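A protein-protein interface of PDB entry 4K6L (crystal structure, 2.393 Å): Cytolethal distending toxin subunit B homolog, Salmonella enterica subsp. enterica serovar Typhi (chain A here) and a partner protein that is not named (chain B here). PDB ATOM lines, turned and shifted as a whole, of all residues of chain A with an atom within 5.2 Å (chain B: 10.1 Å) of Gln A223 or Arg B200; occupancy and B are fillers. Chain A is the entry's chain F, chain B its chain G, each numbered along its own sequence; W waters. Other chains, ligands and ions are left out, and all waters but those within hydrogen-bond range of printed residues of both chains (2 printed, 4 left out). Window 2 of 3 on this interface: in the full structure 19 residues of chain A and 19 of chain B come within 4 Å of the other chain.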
ATOM      1  N   ASP A 217      -4.204   3.986  20.197  1.00  0.00           N
ATOM      2  CA  ASP A 217      -4.649   2.594  20.233  1.00  0.00           C
ATOM      3  C   ASP A 217      -3.568   1.609  19.776  1.00  0.00           C
ATOM      4  O   ASP A 217      -3.570   0.441  20.166  1.00  0.00           O
ATOM      5  CB  ASP A 217      -5.941   2.405  19.430  1.00  0.00           C
ATOM      6  CG  ASP A 217      -6.567   1.042  19.659  1.00  0.00           C
ATOM      7  OD1 ASP A 217      -7.215   0.856  20.716  1.00  0.00           O
ATOM      8  OD2 ASP A 217      -6.399   0.153  18.793  1.00  0.00           O
ATOM      9  N   ALA A 219      -0.645   1.675  20.719  1.00  0.00           N
ATOM     10  CA  ALA A 219       0.224   1.417  21.866  1.00  0.00           C
ATOM     11  C   ALA A 219      -0.009   0.006  22.398  1.00  0.00           C
ATOM     12  O   ALA A 219      -1.141  -0.364  22.699  1.00  0.00           O
ATOM     13  CB  ALA A 219      -0.020   2.435  22.959  1.00  0.00           C
ATOM     14  N   PRO A 220       1.064  -0.789  22.513  1.00  0.00           N
ATOM     15  CA  PRO A 220       0.936  -2.167  23.006  1.00  0.00           C
ATOM     16  C   PRO A 220       0.377  -2.202  24.422  1.00  0.00           C
ATOM     17  O   PRO A 220       0.788  -1.394  25.254  1.00  0.00           O
ATOM     18  CB  PRO A 220       2.380  -2.677  22.995  1.00  0.00           C
ATOM     19  CG  PRO A 220       3.100  -1.779  22.024  1.00  0.00           C
ATOM     20  CD  PRO A 220       2.459  -0.440  22.193  1.00  0.00           C
ATOM     21  N   TYR A 221      -0.558  -3.116  24.671  1.00  0.00           N
ATOM     22  CA  TYR A 221      -1.210  -3.269  25.972  1.00  0.00           C
ATOM     23  C   TYR A 221      -1.910  -1.994  26.460  1.00  0.00           C
ATOM     24  O   TYR A 221      -2.058  -1.771  27.665  1.00  0.00           O
ATOM     25  CB  TYR A 221      -0.228  -3.813  27.020  1.00  0.00           C
ATOM     26  CG  TYR A 221       0.328  -5.175  26.657  1.00  0.00           C
ATOM     27  CD1 TYR A 221      -0.372  -6.340  26.960  1.00  0.00           C
ATOM     28  CD2 TYR A 221       1.549  -5.296  25.997  1.00  0.00           C
ATOM     29  CE1 TYR A 221       0.127  -7.585  26.617  1.00  0.00           C
ATOM     30  CE2 TYR A 221       2.058  -6.537  25.654  1.00  0.00           C
ATOM     31  CZ  TYR A 221       1.346  -7.679  25.964  1.00  0.00           C
ATOM     32  OH  TYR A 221       1.858  -8.916  25.625  1.00  0.00           O
ATOM     33  N   SER A 222      -2.357  -1.176  25.514  1.00  0.00           N
ATOM     34  CA  SER A 222      -3.081   0.051  25.836  1.00  0.00           C
ATOM     35  C   SER A 222      -4.399  -0.225  26.564  1.00  0.00           C
ATOM     36  O   SER A 222      -4.865   0.600  27.346  1.00  0.00           O
ATOM     37  CB  SER A 222      -3.354   0.862  24.562  1.00  0.00           C
ATOM     38  OG  SER A 222      -4.219   0.164  23.682  1.00  0.00           O
ATOM     39  N   GLN A 223      -4.991  -1.388  26.309  1.00  0.00           N
ATOM     40  CA  GLN A 223      -6.270  -1.753  26.924  1.00  0.00           C
ATOM     41  C   GLN A 223      -6.130  -2.147  28.396  1.00  0.00           C
ATOM     42  O   GLN A 223      -7.121  -2.449  29.056  1.00  0.00           O
ATOM     43  CB  GLN A 223      -6.950  -2.888  26.143  1.00  0.00           C
ATOM     44  CG  GLN A 223      -6.339  -4.275  26.362  1.00  0.00           C
ATOM     45  CD  GLN A 223      -4.978  -4.449  25.692  1.00  0.00           C
ATOM     46  OE1 GLN A 223      -4.501  -3.562  24.981  1.00  0.00           O
ATOM     47  NE2 GLN A 223      -4.348  -5.602  25.917  1.00  0.00           N
ATOM     48  N   ARG A 224      -4.904  -2.155  28.910  1.00  0.00           N
ATOM     49  CA  ARG A 224      -4.689  -2.447  30.323  1.00  0.00           C
ATOM     50  C   ARG A 224      -4.823  -1.194  31.174  1.00  0.00           C
ATOM     51  O   ARG A 224      -5.098  -1.271  32.366  1.00  0.00           O
ATOM     52  CB  ARG A 224      -3.312  -3.071  30.548  1.00  0.00           C
ATOM     53  CG  ARG A 224      -3.154  -4.454  29.954  1.00  0.00           C
ATOM     54  CD  ARG A 224      -1.921  -5.131  30.506  1.00  0.00           C
ATOM     55  NE  ARG A 224      -2.029  -5.335  31.946  1.00  0.00           N
ATOM     56  CZ  ARG A 224      -1.000  -5.640  32.729  1.00  0.00           C
ATOM     57  NH1 ARG A 224       0.209  -5.769  32.202  1.00  0.00           N
ATOM     58  NH2 ARG A 224      -1.182  -5.821  34.032  1.00  0.00           N
ATOM     59  N   VAL A 225      -4.620  -0.038  30.553  1.00  0.00           N
ATOM     60  CA  VAL A 225      -4.621   1.220  31.286  1.00  0.00           C
ATOM     61  C   VAL A 225      -6.034   1.611  31.668  1.00  0.00           C
ATOM     62  O   VAL A 225      -6.903   1.783  30.811  1.00  0.00           O
ATOM     63  CB  VAL A 225      -3.968   2.353  30.476  1.00  0.00           C
ATOM     64  CG1 VAL A 225      -3.856   3.612  31.328  1.00  0.00           C
ATOM     65  CG2 VAL A 225      -2.597   1.915  29.965  1.00  0.00           C
ATOM     66  N   ARG A 245      -4.500  -2.601  34.947  1.00  0.00           N
ATOM     67  CA  ARG A 245      -5.388  -3.524  35.635  1.00  0.00           C
ATOM     68  C   ARG A 245      -4.591  -4.728  36.098  1.00  0.00           C
ATOM     69  O   ARG A 245      -3.562  -5.044  35.520  1.00  0.00           O
ATOM     70  CB  ARG A 245      -6.504  -3.996  34.704  1.00  0.00           C
ATOM     71  CG  ARG A 245      -7.423  -2.904  34.207  1.00  0.00           C
ATOM     72  CD  ARG A 245      -8.773  -3.496  33.839  1.00  0.00           C
ATOM     73  NE  ARG A 245      -9.631  -2.522  33.176  1.00  0.00           N
ATOM     74  CZ  ARG A 245      -9.635  -2.315  31.866  1.00  0.00           C
ATOM     75  NH1 ARG A 245      -8.825  -3.019  31.088  1.00  0.00           N
ATOM     76  NH2 ARG A 245     -10.445  -1.408  31.336  1.00  0.00           N
ATOM     77  N   THR B  10       2.175 -18.392  23.388  1.00  0.00           N
ATOM     78  CA  THR B  10       1.599 -17.424  22.472  1.00  0.00           C
ATOM     79  C   THR B  10       2.383 -17.415  21.162  1.00  0.00           C
ATOM     80  O   THR B  10       3.611 -17.292  21.168  1.00  0.00           O
ATOM     81  CB  THR B  10       1.581 -16.022  23.098  1.00  0.00           C
ATOM     82  OG1 THR B  10       0.868 -16.069  24.336  1.00  0.00           O
ATOM     83  CG2 THR B  10       0.894 -15.035  22.184  1.00  0.00           C
ATOM     84  N   ASP B  13       3.101 -14.560  15.639  1.00  0.00           N
ATOM     85  CA  ASP B  13       2.316 -13.506  14.996  1.00  0.00           C
ATOM     86  C   ASP B  13       1.586 -12.632  16.011  1.00  0.00           C
ATOM     87  O   ASP B  13       1.163 -11.518  15.694  1.00  0.00           O
ATOM     88  CB  ASP B  13       1.317 -14.099  13.995  1.00  0.00           C
ATOM     89  CG  ASP B  13       0.237 -14.918  14.670  1.00  0.00           C
ATOM     90  OD1 ASP B  13       0.555 -16.005  15.194  1.00  0.00           O
ATOM     91  OD2 ASP B  13      -0.928 -14.482  14.678  1.00  0.00           O
ATOM     92  N   VAL B  14       1.428 -13.143  17.224  1.00  0.00           N
ATOM     93  CA  VAL B  14       0.819 -12.365  18.297  1.00  0.00           C
ATOM     94  C   VAL B  14       1.883 -11.658  19.132  1.00  0.00           C
ATOM     95  O   VAL B  14       1.767 -10.468  19.407  1.00  0.00           O
ATOM     96  CB  VAL B  14      -0.057 -13.235  19.208  1.00  0.00           C
ATOM     97  CG1 VAL B  14      -0.617 -12.402  20.349  1.00  0.00           C
ATOM     98  CG2 VAL B  14      -1.179 -13.867  18.409  1.00  0.00           C
ATOM     99  N   ILE B  15       2.914 -12.397  19.532  1.00  0.00           N
ATOM    100  CA  ILE B  15       4.006 -11.835  20.328  1.00  0.00           C
ATOM    101  C   ILE B  15       4.753 -10.735  19.573  1.00  0.00           C
ATOM    102  O   ILE B  15       5.048  -9.680  20.142  1.00  0.00           O
ATOM    103  CB  ILE B  15       4.992 -12.922  20.770  1.00  0.00           C
ATOM    104  CG1 ILE B  15       4.297 -13.886  21.731  1.00  0.00           C
ATOM    105  CG2 ILE B  15       6.202 -12.303  21.454  1.00  0.00           C
ATOM    106  CD1 ILE B  15       3.881 -13.240  23.035  1.00  0.00           C
ATOM    107  N   ARG B  17       3.464  -8.859  17.558  1.00  0.00           N
ATOM    108  CA  ARG B  17       2.556  -7.717  17.548  1.00  0.00           C
ATOM    109  C   ARG B  17       2.523  -6.959  18.883  1.00  0.00           C
ATOM    110  O   ARG B  17       2.417  -5.732  18.900  1.00  0.00           O
ATOM    111  CB  ARG B  17       1.137  -8.159  17.159  1.00  0.00           C
ATOM    112  CG  ARG B  17       0.195  -7.010  16.788  1.00  0.00           C
ATOM    113  CD  ARG B  17      -1.271  -7.451  16.823  1.00  0.00           C
ATOM    114  NE  ARG B  17      -1.629  -8.009  18.123  1.00  0.00           N
ATOM    115  CZ  ARG B  17      -2.835  -8.457  18.450  1.00  0.00           C
ATOM    116  NH1 ARG B  17      -3.826  -8.419  17.572  1.00  0.00           N
ATOM    117  NH2 ARG B  17      -3.048  -8.943  19.666  1.00  0.00           N
ATOM    118  N   ASP B  18       2.621  -7.677  19.999  1.00  0.00           N
ATOM    119  CA  ASP B  18       2.392  -7.065  21.311  1.00  0.00           C
ATOM    120  C   ASP B  18       3.633  -6.965  22.197  1.00  0.00           C
ATOM    121  O   ASP B  18       3.762  -6.028  22.980  1.00  0.00           O
ATOM    122  CB  ASP B  18       1.307  -7.827  22.082  1.00  0.00           C
ATOM    123  CG  ASP B  18       0.017  -7.970  21.299  1.00  0.00           C
ATOM    124  OD1 ASP B  18      -0.266  -7.113  20.435  1.00  0.00           O
ATOM    125  OD2 ASP B  18      -0.721  -8.942  21.554  1.00  0.00           O
ATOM    126  N   GLY B  19       4.530  -7.941  22.083  1.00  0.00           N
ATOM    127  CA  GLY B  19       5.646  -8.062  23.004  1.00  0.00           C
ATOM    128  C   GLY B  19       5.188  -8.625  24.338  1.00  0.00           C
ATOM    129  O   GLY B  19       4.082  -9.154  24.446  1.00  0.00           O
ATOM    130  N   SER B  21       4.343  -8.143  28.461  1.00  0.00           N
ATOM    131  CA  SER B  21       3.894  -7.138  29.424  1.00  0.00           C
ATOM    132  C   SER B  21       4.178  -7.533  30.880  1.00  0.00           C
ATOM    133  O   SER B  21       4.106  -8.709  31.240  1.00  0.00           O
ATOM    134  CB  SER B  21       2.396  -6.863  29.230  1.00  0.00           C
ATOM    135  OG  SER B  21       1.942  -5.788  30.029  1.00  0.00           O
ATOM    136  N   LEU B  22       4.501  -6.543  31.713  1.00  0.00           N
ATOM    137  CA  LEU B  22       4.710  -6.774  33.142  1.00  0.00           C
ATOM    138  C   LEU B  22       3.405  -7.197  33.799  1.00  0.00           C
ATOM    139  O   LEU B  22       2.329  -6.824  33.345  1.00  0.00           O
ATOM    140  CB  LEU B  22       5.206  -5.504  33.834  1.00  0.00           C
ATOM    141  CG  LEU B  22       6.446  -4.817  33.269  1.00  0.00           C
ATOM    142  CD1 LEU B  22       6.720  -3.518  34.026  1.00  0.00           C
ATOM    143  CD2 LEU B  22       7.636  -5.741  33.345  1.00  0.00           C
ATOM    144  N   CYS B 196       1.981 -10.791  31.477  1.00  0.00           N
ATOM    145  CA  CYS B 196       0.536 -10.595  31.353  1.00  0.00           C
ATOM    146  C   CYS B 196       0.051 -10.963  29.955  1.00  0.00           C
ATOM    147  O   CYS B 196       0.434 -10.333  28.972  1.00  0.00           O
ATOM    148  CB  CYS B 196       0.149  -9.150  31.695  1.00  0.00           C
ATOM    149  SG  CYS B 196      -1.636  -8.851  31.864  1.00  0.00           S
ATOM    150  N   HIS B 197      -0.789 -11.987  29.872  1.00  0.00           N
ATOM    151  CA  HIS B 197      -1.352 -12.403  28.589  1.00  0.00           C
ATOM    152  C   HIS B 197      -2.644 -11.681  28.248  1.00  0.00           C
ATOM    153  O   HIS B 197      -3.697 -12.300  28.100  1.00  0.00           O
ATOM    154  CB  HIS B 197      -1.548 -13.921  28.535  1.00  0.00           C
ATOM    155  CG  HIS B 197      -0.288 -14.670  28.249  1.00  0.00           C
ATOM    156  ND1 HIS B 197       0.747 -14.760  29.155  1.00  0.00           N
ATOM    157  CD2 HIS B 197       0.123 -15.338  27.145  1.00  0.00           C
ATOM    158  CE1 HIS B 197       1.732 -15.462  28.629  1.00  0.00           C
ATOM    159  NE2 HIS B 197       1.381 -15.822  27.407  1.00  0.00           N
ATOM    160  N   SER B 198      -2.562 -10.362  28.126  1.00  0.00           N
ATOM    161  CA  SER B 198      -3.681  -9.584  27.607  1.00  0.00           C
ATOM    162  C   SER B 198      -3.471  -9.330  26.115  1.00  0.00           C
ATOM    163  O   SER B 198      -2.901  -8.313  25.723  1.00  0.00           O
ATOM    164  CB  SER B 198      -3.825  -8.262  28.360  1.00  0.00           C
ATOM    165  OG  SER B 198      -4.897  -7.495  27.831  1.00  0.00           O
ATOM    166  N   HIS B 199      -3.923 -10.271  25.292  1.00  0.00           N
ATOM    167  CA  HIS B 199      -3.785 -10.163  23.843  1.00  0.00           C
ATOM    168  C   HIS B 199      -5.142  -9.979  23.182  1.00  0.00           C
ATOM    169  O   HIS B 199      -5.969 -10.894  23.174  1.00  0.00           O
ATOM    170  CB  HIS B 199      -3.102 -11.407  23.274  1.00  0.00           C
ATOM    171  CG  HIS B 199      -1.750 -11.675  23.855  1.00  0.00           C
ATOM    172  ND1 HIS B 199      -0.641 -10.915  23.544  1.00  0.00           N
ATOM    173  CD2 HIS B 199      -1.321 -12.630  24.714  1.00  0.00           C
ATOM    174  CE1 HIS B 199       0.409 -11.385  24.195  1.00  0.00           C
ATOM    175  NE2 HIS B 199       0.024 -12.424  24.912  1.00  0.00           N
ATOM    176  N   ARG B 200      -5.366  -8.797  22.618  1.00  0.00           N
ATOM    177  CA  ARG B 200      -6.654  -8.469  22.009  1.00  0.00           C
ATOM    178  C   ARG B 200      -7.001  -9.385  20.837  1.00  0.00           C
ATOM    179  O   ARG B 200      -6.136  -9.732  20.033  1.00  0.00           O
ATOM    180  CB  ARG B 200      -6.681  -7.005  21.582  1.00  0.00           C
ATOM    181  CG  ARG B 200      -6.516  -6.042  22.743  1.00  0.00           C
ATOM    182  CD  ARG B 200      -6.864  -4.624  22.342  1.00  0.00           C
ATOM    183  NE  ARG B 200      -5.900  -4.068  21.401  1.00  0.00           N
ATOM    184  CZ  ARG B 200      -6.011  -2.864  20.854  1.00  0.00           C
ATOM    185  NH1 ARG B 200      -7.052  -2.096  21.151  1.00  0.00           N
ATOM    186  NH2 ARG B 200      -5.089  -2.431  20.009  1.00  0.00           N
ATOM    187  N   GLY B 201      -8.270  -9.792  20.773  1.00  0.00           N
ATOM    188  CA  GLY B 201      -8.762 -10.702  19.750  1.00  0.00           C
ATOM    189  C   GLY B 201      -8.212 -12.118  19.835  1.00  0.00           C
ATOM    190  O   GLY B 201      -8.591 -12.986  19.047  1.00  0.00           O
ATOM    191  N   GLN B 202      -7.322 -12.353  20.797  1.00  0.00           N
ATOM    192  CA  GLN B 202      -6.638 -13.635  20.927  1.00  0.00           C
ATOM    193  C   GLN B 202      -6.937 -14.306  22.262  1.00  0.00           C
ATOM    194  O   GLN B 202      -6.027 -14.542  23.059  1.00  0.00           O
ATOM    195  CB  GLN B 202      -5.122 -13.445  20.790  1.00  0.00           C
ATOM    196  CG  GLN B 202      -4.692 -12.726  19.520  1.00  0.00           C
ATOM    197  CD  GLN B 202      -4.967 -13.538  18.264  1.00  0.00           C
ATOM    198  OE1 GLN B 202      -4.891 -14.767  18.277  1.00  0.00           O
ATOM    199  NE2 GLN B 202      -5.290 -12.850  17.172  1.00  0.00           N
ATOM    200  N   ARG B 203      -8.206 -14.617  22.508  1.00  0.00           N
ATOM    201  CA  ARG B 203      -8.594 -15.238  23.770  1.00  0.00           C
ATOM    202  C   ARG B 203      -8.225 -16.718  23.834  1.00  0.00           C
ATOM    203  O   ARG B 203      -9.092 -17.588  23.776  1.00  0.00           O
ATOM    204  CB  ARG B 203     -10.088 -15.046  24.045  1.00  0.00           C
ATOM    205  CG  ARG B 203     -10.448 -13.658  24.554  1.00  0.00           C
ATOM    206  CD  ARG B 203     -11.920 -13.564  24.930  1.00  0.00           C
ATOM    207  NE  ARG B 203     -12.265 -14.447  26.043  1.00  0.00           N
ATOM    208  CZ  ARG B 203     -13.460 -14.484  26.622  1.00  0.00           C
ATOM    209  NH1 ARG B 203     -14.429 -13.684  26.196  1.00  0.00           N
ATOM    210  NH2 ARG B 203     -13.687 -15.318  27.629  1.00  0.00           N
ATOM    211  N   ALA B 204      -6.931 -16.992  23.957  1.00  0.00           N
ATOM    212  CA  ALA B 204      -6.449 -18.354  24.142  1.00  0.00           C
ATOM    213  C   ALA B 204      -6.044 -18.562  25.596  1.00  0.00           C
ATOM    214  O   ALA B 204      -5.564 -17.636  26.253  1.00  0.00           O
ATOM    215  CB  ALA B 204      -5.276 -18.636  23.218  1.00  0.00           C
HETATM  216  O   HOH W   1      -8.092  -1.721  18.035  1.00  0.00           O
HETATM  217  O   HOH W   2       2.741  -3.453  32.200  1.00  0.00           O
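Water W1 bridges the side-chain carboxylate of Asp A217 (2.6 Å) and the guanidinium group of Arg B200 (3.3 Å). Water W2 lies within hydrogen-bond range of OG of Ser B21 (3.3 Å) and NH1 of Arg A224 (3.4 Å).
CB of Pro A220 touches O of Asp B18 (3.6 Å). Tyr A221 touches Asp B18 (CE2 to O, 3.2 Å). Tyr A221 touches Ser B21. Tyr A221 touches Cys B196. Tyr A221 touches Ser B198 (CE1 to O, 3.2 Å). OH of Tyr A221 touches CE1 of His B199, 3.2 Å away. Arg B200 touches Gln A223 (CG to CD, 3.7 Å).
The backbone carbonyl oxygen (O) of Gln A223 lies within hydrogen-bond range of the guanidinium group (NH1) of Arg A245 (2.7 Å). The guanidinium group (NH2) of Arg A224 lies within hydrogen-bond range of the backbone carbonyl oxygen (O) of Arg A245 (2.9 Å). NE of Arg B17 lies within salt-bridge range of OD1 of Asp B18. NH2 of Arg B17 is in hydrogen-bond range of O of Arg B200, 3.2 Å away. A ring nitrogen (ND1) of His B199 lies within hydrogen-bond range of the side-chain carboxylate (OD2) of Asp B18 (2.8 Å). N of Cys B196 lies within hydrogen-bond range of O of Ser B21 (3.0 Å).
Printed residues of chain B within 4 Å of Tyr A221: Asp B18 (3.2 Å), Gly B19 (2.5 Å), Ser B21 (3.5 Å), Cys B196 (3.6 Å), Ser B198 (3.2 Å) and His B199 (3.2 Å). No residue of chain B comes within 4 Å of Ser A222. Gln A223 touches just these residues of chain B: Ser B198 (2.7 Å) and Arg B200 (3.7 Å). Thr B10 touches none of the printed residues of chain A. Of the printed residues of chain A, Asp B18 touches Pro A220 and Tyr A221. Of the printed residues of chain A, Gly B19 touches Tyr A221 (2.5 Å). Of the printed residues of chain A, His B199 touches Tyr A221. Arg B200 touches just these residues of chain A: Asp A217 and Gln A223. The nearest residue of chain B that does not touch Gln A223 is His B199 (4.7 Å).
Hydrophobic or aromatic side chains of chain B that line the printed part of chain A: His B199. Printed residues of chain A that touch a printed residue of chain B: Asp A217, Pro A220, Tyr A221, Gln A223 and Arg A224. Hydrophobic or aromatic side chains of chain A within 4 Å of the printed part of chain B: Pro A220 and Tyr A221.
The guanidinium group of Arg B200 is in salt-bridge range of the side-chain carboxylate of Asp A217 (3.0 Å). The backbone carbonyl oxygen of Gly B19 is in hydrogen-bond range of the side-chain hydroxyl of Tyr A221. The side-chain amide nitrogen (NE2) of Gln A223 sits at hydrogen-bond distance from the side-chain hydroxyl (OG) of Ser B198 (2.7 Å). NH1 of Arg A224 is in hydrogen-bond range of OG of Ser B21 (2.8 Å). The guanidinium group of Arg A224 lies within hydrogen-bond range of the backbone carbonyl oxygen of Leu B22, at 2.6 Å. The side-chain sulfur (SG) of Cys B196 lies close to the guanidinium group (NE) of Arg A224, 3.5 Å away.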
